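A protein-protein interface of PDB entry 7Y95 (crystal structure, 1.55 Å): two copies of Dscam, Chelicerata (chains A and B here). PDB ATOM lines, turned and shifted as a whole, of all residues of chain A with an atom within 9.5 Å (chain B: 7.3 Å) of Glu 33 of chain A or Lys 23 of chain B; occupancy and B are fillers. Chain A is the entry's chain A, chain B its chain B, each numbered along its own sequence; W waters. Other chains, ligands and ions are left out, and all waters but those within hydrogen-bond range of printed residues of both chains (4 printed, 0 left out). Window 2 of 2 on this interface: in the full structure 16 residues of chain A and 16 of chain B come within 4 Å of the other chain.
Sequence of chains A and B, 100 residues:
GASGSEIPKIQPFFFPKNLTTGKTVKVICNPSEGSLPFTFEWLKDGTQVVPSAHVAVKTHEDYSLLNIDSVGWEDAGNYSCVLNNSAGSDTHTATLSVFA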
ATOM      1  N   SER A   5      11.190 -27.537   9.140  1.00  0.00           N
ATOM      2  CA  SER A   5      10.082 -26.808   8.531  1.00  0.00           C
ATOM      3  C   SER A   5       8.960 -27.813   8.278  1.00  0.00           C
ATOM      4  O   SER A   5       8.997 -28.575   7.306  1.00  0.00           O
ATOM      5  CB  SER A   5      10.532 -26.118   7.249  1.00  0.00           C
ATOM      6  OG  SER A   5       9.470 -25.393   6.669  1.00  0.00           O
ATOM      7  N   GLU A   6       7.960 -27.803   9.154  1.00  0.00           N
ATOM      8  CA  GLU A   6       6.870 -28.770   9.154  1.00  0.00           C
ATOM      9  C   GLU A   6       5.576 -28.057   8.796  1.00  0.00           C
ATOM     10  O   GLU A   6       5.230 -27.050   9.420  1.00  0.00           O
ATOM     11  CB  GLU A   6       6.751 -29.428  10.530  1.00  0.00           C
ATOM     12  CG  GLU A   6       5.997 -30.739  10.566  1.00  0.00           C
ATOM     13  CD  GLU A   6       5.817 -31.266  11.996  1.00  0.00           C
ATOM     14  OE1 GLU A   6       5.660 -32.497  12.163  1.00  0.00           O
ATOM     15  OE2 GLU A   6       5.828 -30.447  12.951  1.00  0.00           O
ATOM     16  N   ILE A   7       4.876 -28.575   7.791  1.00  0.00           N
ATOM     17  CA  ILE A   7       3.600 -27.985   7.374  1.00  0.00           C
ATOM     18  C   ILE A   7       2.612 -28.066   8.532  1.00  0.00           C
ATOM     19  O   ILE A   7       2.638 -29.051   9.303  1.00  0.00           O
ATOM     20  CB  ILE A   7       3.065 -28.710   6.126  1.00  0.00           C
ATOM     21  CG1 ILE A   7       3.803 -28.201   4.877  1.00  0.00           C
ATOM     22  CG2 ILE A   7       1.578 -28.509   5.959  1.00  0.00           C
ATOM     23  CD1 ILE A   7       3.693 -29.091   3.669  1.00  0.00           C
ATOM     24  N   PRO A   8       1.737 -27.083   8.725  1.00  0.00           N
ATOM     25  CA  PRO A   8       0.824 -27.156   9.871  1.00  0.00           C
ATOM     26  C   PRO A   8      -0.333 -28.111   9.646  1.00  0.00           C
ATOM     27  O   PRO A   8      -0.750 -28.381   8.516  1.00  0.00           O
ATOM     28  CB  PRO A   8       0.327 -25.714  10.023  1.00  0.00           C
ATOM     29  CG  PRO A   8       0.441 -25.135   8.648  1.00  0.00           C
ATOM     30  CD  PRO A   8       1.631 -25.805   7.991  1.00  0.00           C
ATOM     31  N   LYS A   9      -0.854 -28.619  10.759  1.00  0.00           N
ATOM     32  CA  LYS A   9      -2.026 -29.482  10.758  1.00  0.00           C
ATOM     33  C   LYS A   9      -2.959 -28.979  11.840  1.00  0.00           C
ATOM     34  O   LYS A   9      -2.554 -28.892  13.004  1.00  0.00           O
ATOM     35  CB  LYS A   9      -1.636 -30.936  11.013  1.00  0.00           C
ATOM     36  CG  LYS A   9      -2.770 -31.908  10.789  1.00  0.00           C
ATOM     37  CD  LYS A   9      -2.385 -33.317  11.194  1.00  0.00           C
ATOM     38  CE  LYS A   9      -3.578 -34.254  11.044  1.00  0.00           C
ATOM     39  NZ  LYS A   9      -3.236 -35.659  11.388  1.00  0.00           N
ATOM     40  N   ILE A  10      -4.186 -28.621  11.458  1.00  0.00           N
ATOM     41  CA  ILE A  10      -5.143 -28.077  12.411  1.00  0.00           C
ATOM     42  C   ILE A  10      -5.746 -29.219  13.200  1.00  0.00           C
ATOM     43  O   ILE A  10      -6.083 -30.272  12.647  1.00  0.00           O
ATOM     44  CB  ILE A  10      -6.239 -27.269  11.698  1.00  0.00           C
ATOM     45  CG1 ILE A  10      -5.710 -25.921  11.212  1.00  0.00           C
ATOM     46  CG2 ILE A  10      -7.414 -26.999  12.625  1.00  0.00           C
ATOM     47  CD1 ILE A  10      -6.718 -25.136  10.388  1.00  0.00           C
ATOM     48  N   GLN A  11      -5.891 -29.008  14.492  1.00  0.00           N
ATOM     49  CA  GLN A  11      -6.688 -29.895  15.334  1.00  0.00           C
ATOM     50  C   GLN A  11      -8.162 -29.683  15.004  1.00  0.00           C
ATOM     51  O   GLN A  11      -8.637 -28.538  15.057  1.00  0.00           O
ATOM     52  CB  GLN A  11      -6.414 -29.596  16.809  1.00  0.00           C
ATOM     53  CG  GLN A  11      -7.287 -30.376  17.749  1.00  0.00           C
ATOM     54  CD  GLN A  11      -7.000 -30.060  19.208  1.00  0.00           C
ATOM     55  OE1 GLN A  11      -5.850 -30.034  19.634  1.00  0.00           O
ATOM     56  NE2 GLN A  11      -8.050 -29.853  19.985  1.00  0.00           N
ATOM     57  N   PRO A  12      -8.910 -30.718  14.645  1.00  0.00           N
ATOM     58  CA  PRO A  12     -10.318 -30.502  14.284  1.00  0.00           C
ATOM     59  C   PRO A  12     -11.106 -29.943  15.459  1.00  0.00           C
ATOM     60  O   PRO A  12     -10.996 -30.424  16.586  1.00  0.00           O
ATOM     61  CB  PRO A  12     -10.810 -31.899  13.884  1.00  0.00           C
ATOM     62  CG  PRO A  12      -9.591 -32.700  13.655  1.00  0.00           C
ATOM     63  CD  PRO A  12      -8.509 -32.132  14.526  1.00  0.00           C
ATOM     64  N   ASN A  30      -6.127 -24.553  16.649  1.00  0.00           N
ATOM     65  CA  ASN A  30      -4.736 -24.687  17.052  1.00  0.00           C
ATOM     66  C   ASN A  30      -4.067 -25.771  16.230  1.00  0.00           C
ATOM     67  O   ASN A  30      -4.732 -26.715  15.787  1.00  0.00           O
ATOM     68  CB  ASN A  30      -4.603 -25.004  18.553  1.00  0.00           C
ATOM     69  CG  ASN A  30      -5.214 -26.336  18.928  1.00  0.00           C
ATOM     70  OD1 ASN A  30      -6.421 -26.429  19.152  1.00  0.00           O
ATOM     71  ND2 ASN A  30      -4.380 -27.375  19.013  1.00  0.00           N
ATOM     72  N   PRO A  31      -2.764 -25.655  15.989  1.00  0.00           N
ATOM     73  CA  PRO A  31      -2.048 -26.747  15.324  1.00  0.00           C
ATOM     74  C   PRO A  31      -1.844 -27.914  16.273  1.00  0.00           C
ATOM     75  O   PRO A  31      -1.592 -27.731  17.467  1.00  0.00           O
ATOM     76  CB  PRO A  31      -0.712 -26.110  14.924  1.00  0.00           C
ATOM     77  CG  PRO A  31      -0.552 -24.975  15.880  1.00  0.00           C
ATOM     78  CD  PRO A  31      -1.918 -24.456  16.160  1.00  0.00           C
ATOM     79  N   SER A  32      -1.974 -29.121  15.729  1.00  0.00           N
ATOM     80  CA  SER A  32      -1.462 -30.315  16.382  1.00  0.00           C
ATOM     81  C   SER A  32      -0.027 -30.594  15.971  1.00  0.00           C
ATOM     82  O   SER A  32       0.699 -31.270  16.710  1.00  0.00           O
ATOM     83  CB  SER A  32      -2.333 -31.525  16.036  1.00  0.00           C
ATOM     84  OG  SER A  32      -2.187 -31.832  14.665  1.00  0.00           O
ATOM     85  N   GLU A  33       0.374 -30.099  14.800  1.00  0.00           N
ATOM     86  CA  GLU A  33       1.722 -30.246  14.283  1.00  0.00           C
ATOM     87  C   GLU A  33       2.053 -29.001  13.480  1.00  0.00           C
ATOM     88  O   GLU A  33       1.163 -28.282  13.017  1.00  0.00           O
ATOM     89  CB  GLU A  33       1.882 -31.476  13.382  1.00  0.00           C
ATOM     90  CG  GLU A  33       1.333 -32.754  13.941  1.00  0.00           C
ATOM     91  CD  GLU A  33       1.415 -33.885  12.930  1.00  0.00           C
ATOM     92  OE1 GLU A  33       1.610 -33.593  11.724  1.00  0.00           O
ATOM     93  OE2 GLU A  33       1.285 -35.061  13.338  1.00  0.00           O
ATOM     94  N   GLY A  34       3.346 -28.761  13.305  1.00  0.00           N
ATOM     95  CA  GLY A  34       3.814 -27.666  12.473  1.00  0.00           C
ATOM     96  C   GLY A  34       4.865 -26.832  13.177  1.00  0.00           C
ATOM     97  O   GLY A  34       4.898 -26.736  14.405  1.00  0.00           O
ATOM     98  N   SER A  35       5.729 -26.205  12.385  1.00  0.00           N
ATOM     99  CA  SER A  35       6.747 -25.323  12.932  1.00  0.00           C
ATOM    100  C   SER A  35       6.171 -23.931  13.173  1.00  0.00           C
ATOM    101  O   SER A  35       5.252 -23.483  12.484  1.00  0.00           O
ATOM    102  CB  SER A  35       7.946 -25.238  11.988  1.00  0.00           C
ATOM    103  OG  SER A  35       7.513 -25.234  10.639  1.00  0.00           O
ATOM    104  N   LEU A  36       6.707 -23.257  14.182  1.00  0.00           N
ATOM    105  CA  LEU A  36       6.400 -21.858  14.401  1.00  0.00           C
ATOM    106  C   LEU A  36       6.984 -21.025  13.265  1.00  0.00           C
ATOM    107  O   LEU A  36       7.847 -21.495  12.519  1.00  0.00           O
ATOM    108  CB  LEU A  36       6.973 -21.392  15.737  1.00  0.00           C
ATOM    109  CG  LEU A  36       6.271 -21.918  16.992  1.00  0.00           C
ATOM    110  CD1 LEU A  36       7.193 -21.827  18.202  1.00  0.00           C
ATOM    111  CD2 LEU A  36       4.975 -21.162  17.254  1.00  0.00           C
ATOM    112  N   PRO A  37       6.505 -19.787  13.089  1.00  0.00           N
ATOM    113  CA  PRO A  37       5.370 -19.164  13.782  1.00  0.00           C
ATOM    114  C   PRO A  37       4.072 -19.401  13.028  1.00  0.00           C
ATOM    115  O   PRO A  37       4.098 -19.768  11.850  1.00  0.00           O
ATOM    116  CB  PRO A  37       5.732 -17.681  13.782  1.00  0.00           C
ATOM    117  CG  PRO A  37       6.484 -17.503  12.477  1.00  0.00           C
ATOM    118  CD  PRO A  37       7.154 -18.847  12.154  1.00  0.00           C
ATOM    119  N   PHE A  38       2.950 -19.175  13.695  1.00  0.00           N
ATOM    120  CA  PHE A  38       1.640 -19.430  13.122  1.00  0.00           C
ATOM    121  C   PHE A  38       0.858 -18.136  12.959  1.00  0.00           C
ATOM    122  O   PHE A  38       0.949 -17.231  13.796  1.00  0.00           O
ATOM    123  CB  PHE A  38       0.832 -20.392  14.006  1.00  0.00           C
ATOM    124  CG  PHE A  38       1.475 -21.730  14.185  1.00  0.00           C
ATOM    125  CD1 PHE A  38       1.478 -22.651  13.152  1.00  0.00           C
ATOM    126  CD2 PHE A  38       2.078 -22.072  15.375  1.00  0.00           C
ATOM    127  CE1 PHE A  38       2.074 -23.876  13.309  1.00  0.00           C
ATOM    128  CE2 PHE A  38       2.667 -23.300  15.540  1.00  0.00           C
ATOM    129  CZ  PHE A  38       2.671 -24.205  14.507  1.00  0.00           C
ATOM    130  N   PHE A  40      -3.311 -17.050  12.051  1.00  0.00           N
ATOM    131  CA  PHE A  40      -4.669 -17.563  12.082  1.00  0.00           C
ATOM    132  C   PHE A  40      -5.610 -16.574  11.408  1.00  0.00           C
ATOM    133  O   PHE A  40      -5.496 -15.361  11.606  1.00  0.00           O
ATOM    134  CB  PHE A  40      -5.158 -17.786  13.529  1.00  0.00           C
ATOM    135  CG  PHE A  40      -4.345 -18.774  14.310  1.00  0.00           C
ATOM    136  CD1 PHE A  40      -3.163 -18.394  14.931  1.00  0.00           C
ATOM    137  CD2 PHE A  40      -4.788 -20.080  14.463  1.00  0.00           C
ATOM    138  CE1 PHE A  40      -2.425 -19.303  15.653  1.00  0.00           C
ATOM    139  CE2 PHE A  40      -4.054 -20.983  15.184  1.00  0.00           C
ATOM    140  CZ  PHE A  40      -2.870 -20.603  15.773  1.00  0.00           C
ATOM    141  N   ASP A  62       0.066 -19.783  19.503  1.00  0.00           N
ATOM    142  CA  ASP A  62      -0.168 -21.150  19.039  1.00  0.00           C
ATOM    143  C   ASP A  62      -1.635 -21.572  19.115  1.00  0.00           C
ATOM    144  O   ASP A  62      -1.940 -22.769  18.996  1.00  0.00           O
ATOM    145  CB  ASP A  62       0.707 -22.131  19.825  1.00  0.00           C
ATOM    146  CG  ASP A  62       0.352 -22.183  21.294  1.00  0.00           C
ATOM    147  OD1 ASP A  62      -0.412 -21.316  21.761  1.00  0.00           O
ATOM    148  OD2 ASP A  62       0.844 -23.105  21.985  1.00  0.00           O
ATOM    149  N   LEU A  83      -4.924 -21.729   8.949  1.00  0.00           N
ATOM    150  CA  LEU A  83      -3.695 -21.739   9.725  1.00  0.00           C
ATOM    151  C   LEU A  83      -2.514 -21.874   8.783  1.00  0.00           C
ATOM    152  O   LEU A  83      -2.478 -22.793   7.963  1.00  0.00           O
ATOM    153  CB  LEU A  83      -3.716 -22.903  10.716  1.00  0.00           C
ATOM    154  CG  LEU A  83      -2.428 -23.192  11.474  1.00  0.00           C
ATOM    155  CD1 LEU A  83      -2.217 -22.107  12.498  1.00  0.00           C
ATOM    156  CD2 LEU A  83      -2.499 -24.566  12.120  1.00  0.00           C
ATOM    157  N   ASN A  84      -1.549 -20.963   8.919  1.00  0.00           N
ATOM    158  CA  ASN A  84      -0.354 -20.949   8.093  1.00  0.00           C
ATOM    159  C   ASN A  84       0.889 -20.832   8.966  1.00  0.00           C
ATOM    160  O   ASN A  84       0.836 -20.341  10.097  1.00  0.00           O
ATOM    161  CB  ASN A  84      -0.370 -19.779   7.091  1.00  0.00           C
ATOM    162  CG  ASN A  84      -1.668 -19.695   6.294  1.00  0.00           C
ATOM    163  OD1 ASN A  84      -2.371 -20.684   6.122  1.00  0.00           O
ATOM    164  ND2 ASN A  84      -1.982 -18.501   5.800  1.00  0.00           N
ATOM    165  N   ASN A  85       2.020 -21.286   8.422  1.00  0.00           N
ATOM    166  CA  ASN A  85       3.333 -20.998   8.990  1.00  0.00           C
ATOM    167  C   ASN A  85       4.195 -20.717   7.765  1.00  0.00           C
ATOM    168  O   ASN A  85       3.669 -20.325   6.717  1.00  0.00           O
ATOM    169  CB  ASN A  85       3.891 -22.109   9.877  1.00  0.00           C
ATOM    170  CG  ASN A  85       3.997 -23.434   9.188  1.00  0.00           C
ATOM    171  OD1 ASN A  85       3.899 -23.543   7.968  1.00  0.00           O
ATOM    172  ND2 ASN A  85       4.192 -24.476   9.990  1.00  0.00           N
ATOM    173  N   ALA A  87       5.922 -22.993   6.149  1.00  0.00           N
ATOM    174  CA  ALA A  87       5.992 -24.203   5.342  1.00  0.00           C
ATOM    175  C   ALA A  87       4.726 -24.459   4.542  1.00  0.00           C
ATOM    176  O   ALA A  87       4.809 -24.986   3.431  1.00  0.00           O
ATOM    177  CB  ALA A  87       6.269 -25.423   6.232  1.00  0.00           C
ATOM    178  N   GLY A  88       3.562 -24.131   5.090  1.00  0.00           N
ATOM    179  CA  GLY A  88       2.323 -24.407   4.390  1.00  0.00           C
ATOM    180  C   GLY A  88       1.123 -23.888   5.148  1.00  0.00           C
ATOM    181  O   GLY A  88       1.249 -23.090   6.078  1.00  0.00           O
ATOM    182  N   SER A  89      -0.050 -24.335   4.706  1.00  0.00           N
ATOM    183  CA  SER A  89      -1.314 -23.904   5.276  1.00  0.00           C
ATOM    184  C   SER A  89      -2.250 -25.098   5.415  1.00  0.00           C
ATOM    185  O   SER A  89      -2.119 -26.110   4.725  1.00  0.00           O
ATOM    186  CB  SER A  89      -1.978 -22.825   4.416  1.00  0.00           C
ATOM    187  OG  SER A  89      -2.251 -23.325   3.128  1.00  0.00           O
ATOM    188  N   ASP A  90      -3.201 -24.961   6.333  1.00  0.00           N
ATOM    189  CA  ASP A  90      -4.241 -25.951   6.560  1.00  0.00           C
ATOM    190  C   ASP A  90      -5.516 -25.196   6.899  1.00  0.00           C
ATOM    191  O   ASP A  90      -5.481 -24.034   7.311  1.00  0.00           O
ATOM    192  CB  ASP A  90      -3.865 -26.920   7.690  1.00  0.00           C
ATOM    193  CG  ASP A  90      -4.744 -28.160   7.726  1.00  0.00           C
ATOM    194  OD1 ASP A  90      -5.341 -28.541   6.692  1.00  0.00           O
ATOM    195  OD2 ASP A  90      -4.854 -28.754   8.812  1.00  0.00           O
ATOM    196  N   PRO B  16      -9.669 -34.727  20.410  1.00  0.00           N
ATOM    197  CA  PRO B  16      -9.660 -35.185  19.020  1.00  0.00           C
ATOM    198  C   PRO B  16      -9.588 -36.700  18.946  1.00  0.00           C
ATOM    199  O   PRO B  16      -9.065 -37.364  19.844  1.00  0.00           O
ATOM    200  CB  PRO B  16      -8.401 -34.535  18.437  1.00  0.00           C
ATOM    201  CG  PRO B  16      -8.084 -33.417  19.354  1.00  0.00           C
ATOM    202  CD  PRO B  16      -8.530 -33.850  20.719  1.00  0.00           C
ATOM    203  N   ASN B  18      -7.950 -38.268  16.494  1.00  0.00           N
ATOM    204  CA  ASN B  18      -6.815 -38.601  15.642  1.00  0.00           C
ATOM    205  C   ASN B  18      -5.484 -38.387  16.355  1.00  0.00           C
ATOM    206  O   ASN B  18      -4.471 -38.102  15.713  1.00  0.00           O
ATOM    207  CB  ASN B  18      -6.857 -37.783  14.353  1.00  0.00           C
ATOM    208  CG  ASN B  18      -6.537 -36.320  14.573  1.00  0.00           C
ATOM    209  OD1 ASN B  18      -6.687 -35.798  15.678  1.00  0.00           O
ATOM    210  ND2 ASN B  18      -6.085 -35.649  13.514  1.00  0.00           N
ATOM    211  N   LEU B  19      -5.455 -38.542  17.677  1.00  0.00           N
ATOM    212  CA  LEU B  19      -4.249 -38.228  18.435  1.00  0.00           C
ATOM    213  C   LEU B  19      -3.218 -39.334  18.249  1.00  0.00           C
ATOM    214  O   LEU B  19      -3.493 -40.502  18.527  1.00  0.00           O
ATOM    215  CB  LEU B  19      -4.569 -38.048  19.917  1.00  0.00           C
ATOM    216  CG  LEU B  19      -5.383 -36.824  20.273  1.00  0.00           C
ATOM    217  CD1 LEU B  19      -5.504 -36.713  21.787  1.00  0.00           C
ATOM    218  CD2 LEU B  19      -4.767 -35.565  19.709  1.00  0.00           C
ATOM    219  N   THR B  20      -2.034 -38.962  17.776  1.00  0.00           N
ATOM    220  CA  THR B  20      -0.890 -39.844  17.668  1.00  0.00           C
ATOM    221  C   THR B  20       0.221 -39.317  18.564  1.00  0.00           C
ATOM    222  O   THR B  20       0.288 -38.124  18.873  1.00  0.00           O
ATOM    223  CB  THR B  20      -0.407 -39.948  16.214  1.00  0.00           C
ATOM    224  OG1 THR B  20      -0.174 -38.640  15.684  1.00  0.00           O
ATOM    225  CG2 THR B  20      -1.453 -40.641  15.370  1.00  0.00           C
ATOM    226  N   THR B  21       1.099 -40.222  18.976  1.00  0.00           N
ATOM    227  CA  THR B  21       2.213 -39.850  19.837  1.00  0.00           C
ATOM    228  C   THR B  21       3.008 -38.709  19.219  1.00  0.00           C
ATOM    229  O   THR B  21       3.430 -38.780  18.060  1.00  0.00           O
ATOM    230  CB  THR B  21       3.125 -41.056  20.077  1.00  0.00           C
ATOM    231  OG1 THR B  21       2.400 -42.078  20.773  1.00  0.00           O
ATOM    232  CG2 THR B  21       4.338 -40.647  20.904  1.00  0.00           C
ATOM    233  N   GLY B  22       3.197 -37.647  19.999  1.00  0.00           N
ATOM    234  CA  GLY B  22       3.949 -36.495  19.583  1.00  0.00           C
ATOM    235  C   GLY B  22       3.114 -35.284  19.231  1.00  0.00           C
ATOM    236  O   GLY B  22       3.661 -34.179  19.155  1.00  0.00           O
ATOM    237  N   LYS B  23       1.819 -35.460  18.997  1.00  0.00           N
ATOM    238  CA  LYS B  23       0.972 -34.328  18.657  1.00  0.00           C
ATOM    239  C   LYS B  23       0.791 -33.407  19.858  1.00  0.00           C
ATOM    240  O   LYS B  23       0.838 -33.832  21.013  1.00  0.00           O
ATOM    241  CB  LYS B  23      -0.403 -34.795  18.178  1.00  0.00           C
ATOM    242  CG  LYS B  23      -0.513 -35.127  16.702  1.00  0.00           C
ATOM    243  CD  LYS B  23      -1.969 -35.427  16.336  1.00  0.00           C
ATOM    244  CE  LYS B  23      -2.178 -35.628  14.841  1.00  0.00           C
ATOM    245  NZ  LYS B  23      -0.903 -35.808  14.103  1.00  0.00           N
ATOM    246  N   THR B  24       0.599 -32.125  19.569  1.00  0.00           N
ATOM    247  CA  THR B  24       0.076 -31.189  20.551  1.00  0.00           C
ATOM    248  C   THR B  24      -1.444 -31.299  20.586  1.00  0.00           C
ATOM    249  O   THR B  24      -2.091 -31.440  19.548  1.00  0.00           O
ATOM    250  CB  THR B  24       0.478 -29.756  20.201  1.00  0.00           C
ATOM    251  OG1 THR B  24       1.898 -29.630  20.278  1.00  0.00           O
ATOM    252  CG2 THR B  24      -0.169 -28.764  21.171  1.00  0.00           C
ATOM    253  N   VAL B  25      -2.023 -31.234  21.780  1.00  0.00           N
ATOM    254  CA  VAL B  25      -3.470 -31.247  21.927  1.00  0.00           C
ATOM    255  C   VAL B  25      -3.868 -30.146  22.900  1.00  0.00           C
ATOM    256  O   VAL B  25      -3.226 -29.957  23.940  1.00  0.00           O
ATOM    257  CB  VAL B  25      -3.987 -32.629  22.388  1.00  0.00           C
ATOM    258  CG1 VAL B  25      -3.375 -33.023  23.695  1.00  0.00           C
ATOM    259  CG2 VAL B  25      -5.514 -32.625  22.462  1.00  0.00           C
ATOM    260  N   ILE B  68      -1.354 -30.051  26.177  1.00  0.00           N
ATOM    261  CA  ILE B  68      -0.406 -31.147  26.313  1.00  0.00           C
ATOM    262  C   ILE B  68       0.457 -31.162  25.063  1.00  0.00           C
ATOM    263  O   ILE B  68      -0.054 -31.369  23.954  1.00  0.00           O
ATOM    264  CB  ILE B  68      -1.113 -32.498  26.503  1.00  0.00           C
ATOM    265  CG1 ILE B  68      -1.985 -32.465  27.757  1.00  0.00           C
ATOM    266  CG2 ILE B  68      -0.095 -33.623  26.595  1.00  0.00           C
ATOM    267  CD1 ILE B  68      -2.850 -33.692  27.944  1.00  0.00           C
ATOM    268  N   ASP B  69       1.745 -30.900  25.229  1.00  0.00           N
ATOM    269  CA  ASP B  69       2.711 -31.049  24.156  1.00  0.00           C
ATOM    270  C   ASP B  69       3.186 -32.495  24.106  1.00  0.00           C
ATOM    271  O   ASP B  69       3.235 -33.189  25.127  1.00  0.00           O
ATOM    272  CB  ASP B  69       3.900 -30.112  24.370  1.00  0.00           C
ATOM    273  CG  ASP B  69       3.491 -28.647  24.390  1.00  0.00           C
ATOM    274  OD1 ASP B  69       2.679 -28.243  23.522  1.00  0.00           O
ATOM    275  OD2 ASP B  69       3.974 -27.906  25.274  1.00  0.00           O
ATOM    276  N   SER B  70       3.541 -32.940  22.908  1.00  0.00           N
ATOM    277  CA  SER B  70       4.067 -34.282  22.674  1.00  0.00           C
ATOM    278  C   SER B  70       3.267 -35.325  23.447  1.00  0.00           C
ATOM    279  O   SER B  70       3.781 -36.041  24.304  1.00  0.00           O
ATOM    280  CB  SER B  70       5.549 -34.356  23.032  1.00  0.00           C
ATOM    281  OG  SER B  70       6.277 -33.341  22.363  1.00  0.00           O
ATOM    282  N   VAL B  71       1.975 -35.398  23.128  1.00  0.00           N
ATOM    283  CA  VAL B  71       1.104 -36.330  23.824  1.00  0.00           C
ATOM    284  C   VAL B  71       1.622 -37.754  23.651  1.00  0.00           C
ATOM    285  O   VAL B  71       2.229 -38.105  22.629  1.00  0.00           O
ATOM    286  CB  VAL B  71      -0.341 -36.189  23.316  1.00  0.00           C
ATOM    287  CG1 VAL B  71      -0.505 -36.807  21.931  1.00  0.00           C
ATOM    288  CG2 VAL B  71      -1.313 -36.801  24.301  1.00  0.00           C
ATOM    289  N   GLY B  72       1.389 -38.582  24.673  1.00  0.00           N
ATOM    290  CA  GLY B  72       1.777 -39.977  24.634  1.00  0.00           C
ATOM    291  C   GLY B  72       0.754 -40.830  25.353  1.00  0.00           C
ATOM    292  O   GLY B  72      -0.255 -40.328  25.850  1.00  0.00           O
ATOM    293  N   ASP B  75      -0.588 -39.892  28.787  1.00  0.00           N
ATOM    294  CA  ASP B  75      -1.567 -38.821  28.905  1.00  0.00           C
ATOM    295  C   ASP B  75      -2.998 -39.302  28.714  1.00  0.00           C
ATOM    296  O   ASP B  75      -3.931 -38.541  28.994  1.00  0.00           O
ATOM    297  CB  ASP B  75      -1.270 -37.723  27.886  1.00  0.00           C
ATOM    298  CG  ASP B  75       0.094 -37.104  28.082  1.00  0.00           C
ATOM    299  OD1 ASP B  75       0.338 -36.530  29.167  1.00  0.00           O
ATOM    300  OD2 ASP B  75       0.927 -37.196  27.149  1.00  0.00           O
HETATM  301  O   HOH W   1       2.126 -26.122  22.108  1.00  0.00           O
HETATM  302  O   HOH W   2      -4.560 -32.227  18.644  1.00  0.00           O
HETATM  303  O   HOH W   3      -4.633 -32.872  13.994  1.00  0.00           O
HETATM  304  O   HOH W   4       3.573 -31.944  17.165  1.00  0.00           O
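The backbone carbonyl oxygen (O) of Ser 32 of chain A is in hydrogen-bond range of the backbone NH (N) of Thr 24 of chain B (3.0 Å).
The side-chain amino group (NZ) of Lys 23 of chain B lies within salt-bridge range of the side-chain carboxylate (OE2) of Glu 33 of chain A (2.4 Å).
No position is printed for both chains.
Of the 8 pairs that touch across the chains among the printed residues, none has its exchanged pair printed and touching as well.
Ser 5 of chain A touches none of the printed residues of chain B.
Printed residues of chain B within 4 Å of Gln 11 of chain A: Pro 16 (3.5 Å) and Val 25 (3.5 Å).
Printed residues of chain B within 4 Å of Pro 31 of chain A: Thr 24.
Printed residues of chain A within 4 Å of Asn 18 of chain B: Lys 9 (3.6 Å).
No residue of chain A comes within 4 Å of Thr 20 of chain B.
No residue of chain A comes within 4 Å of Gly 22 of chain B.
Of the printed residues of chain A, Val 25 of chain B touches Gln 11 (3.5 Å).
Asp 69 of chain B touches none of the printed residues of chain A.
The nearest residue of chain B that does not touch Glu 33 of chain A is Thr 20 of chain B (4.5 Å).
Of the 15 printed residues of chain B, 5 touch a printed residue of chain A.
Hydrophobic or aromatic side chains of chain B that line the printed part of chain A: Pro 16 and Val 25.
Along chain A the printed residues that touch a printed residue of chain B span positions 9 to 33.
Among the printed residues, 8 pairs touch across the chains.
Among the printed residues, Asp or Glu carboxylates within 4 Å of a Lys or Arg side-chain nitrogen of the other chain: Glu 33 of chain A with Lys 23 of chain B (2.4 Å).
Among the printed residues, pairs that only touch across the chains: Lys 9 of chain A with Asn 18 of chain B (3.6 Å), Lys 9 of chain A with Lys 23 of chain B (3.6 Å), Gln 11 of chain A with Pro 16 of chain B (3.5 Å), Gln 11 of chain A with Val 25 of chain B (3.5 Å), Pro 31 of chain A with Thr 24 of chain B (3.98 Å) and Ser 32 of chain A with Lys 23 of chain B (3.6 Å).
Water W1 bridges the side-chain carboxylate of Asp 69 of chain B (2.6 Å) and the side-chain carboxylate of Asp 62 of chain A (3.3 Å).
Water W2 lies within hydrogen-bond range of the side-chain amide oxygen of Gln 11 of chain A (2.7 Å) and the backbone carbonyl oxygen of Thr 24 of chain B (2.7 Å).
Water W3 lies within hydrogen-bond range of the side-chain hydroxyl (OG) of Ser 32 of chain A (2.7 Å), the side-chain amide nitrogen (ND2) of Asn 18 of chain B (3.2 Å) and the backbone carbonyl oxygen (O) of Ile 10 of chain A (3.3 Å).
The backbone carbonyl oxygen of Lys 23 of chain B is in hydrogen-bond range of the backbone NH of Ser 70 of chain B (3.4 Å).
O of Lys 9 of chain A sits at hydrogen-bond distance from N of Ser 32 of chain A, at 2.8 Å.
OG1 of Thr 20 of chain B sits at hydrogen-bond distance from NZ of Lys 23 of chain B, 3.3 Å away.
The backbone carbonyl oxygen (O) of Val 25 of chain B sits at hydrogen-bond distance from the backbone NH (N) of Ile 68 of chain B (2.9 Å).
O of Lys 23 of chain B lies within hydrogen-bond range of N of Val 71 of chain B, at 2.9 Å.
N of Lys 9 of chain A is in hydrogen-bond range of O of Glu 33 of chain A (3.0 Å).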
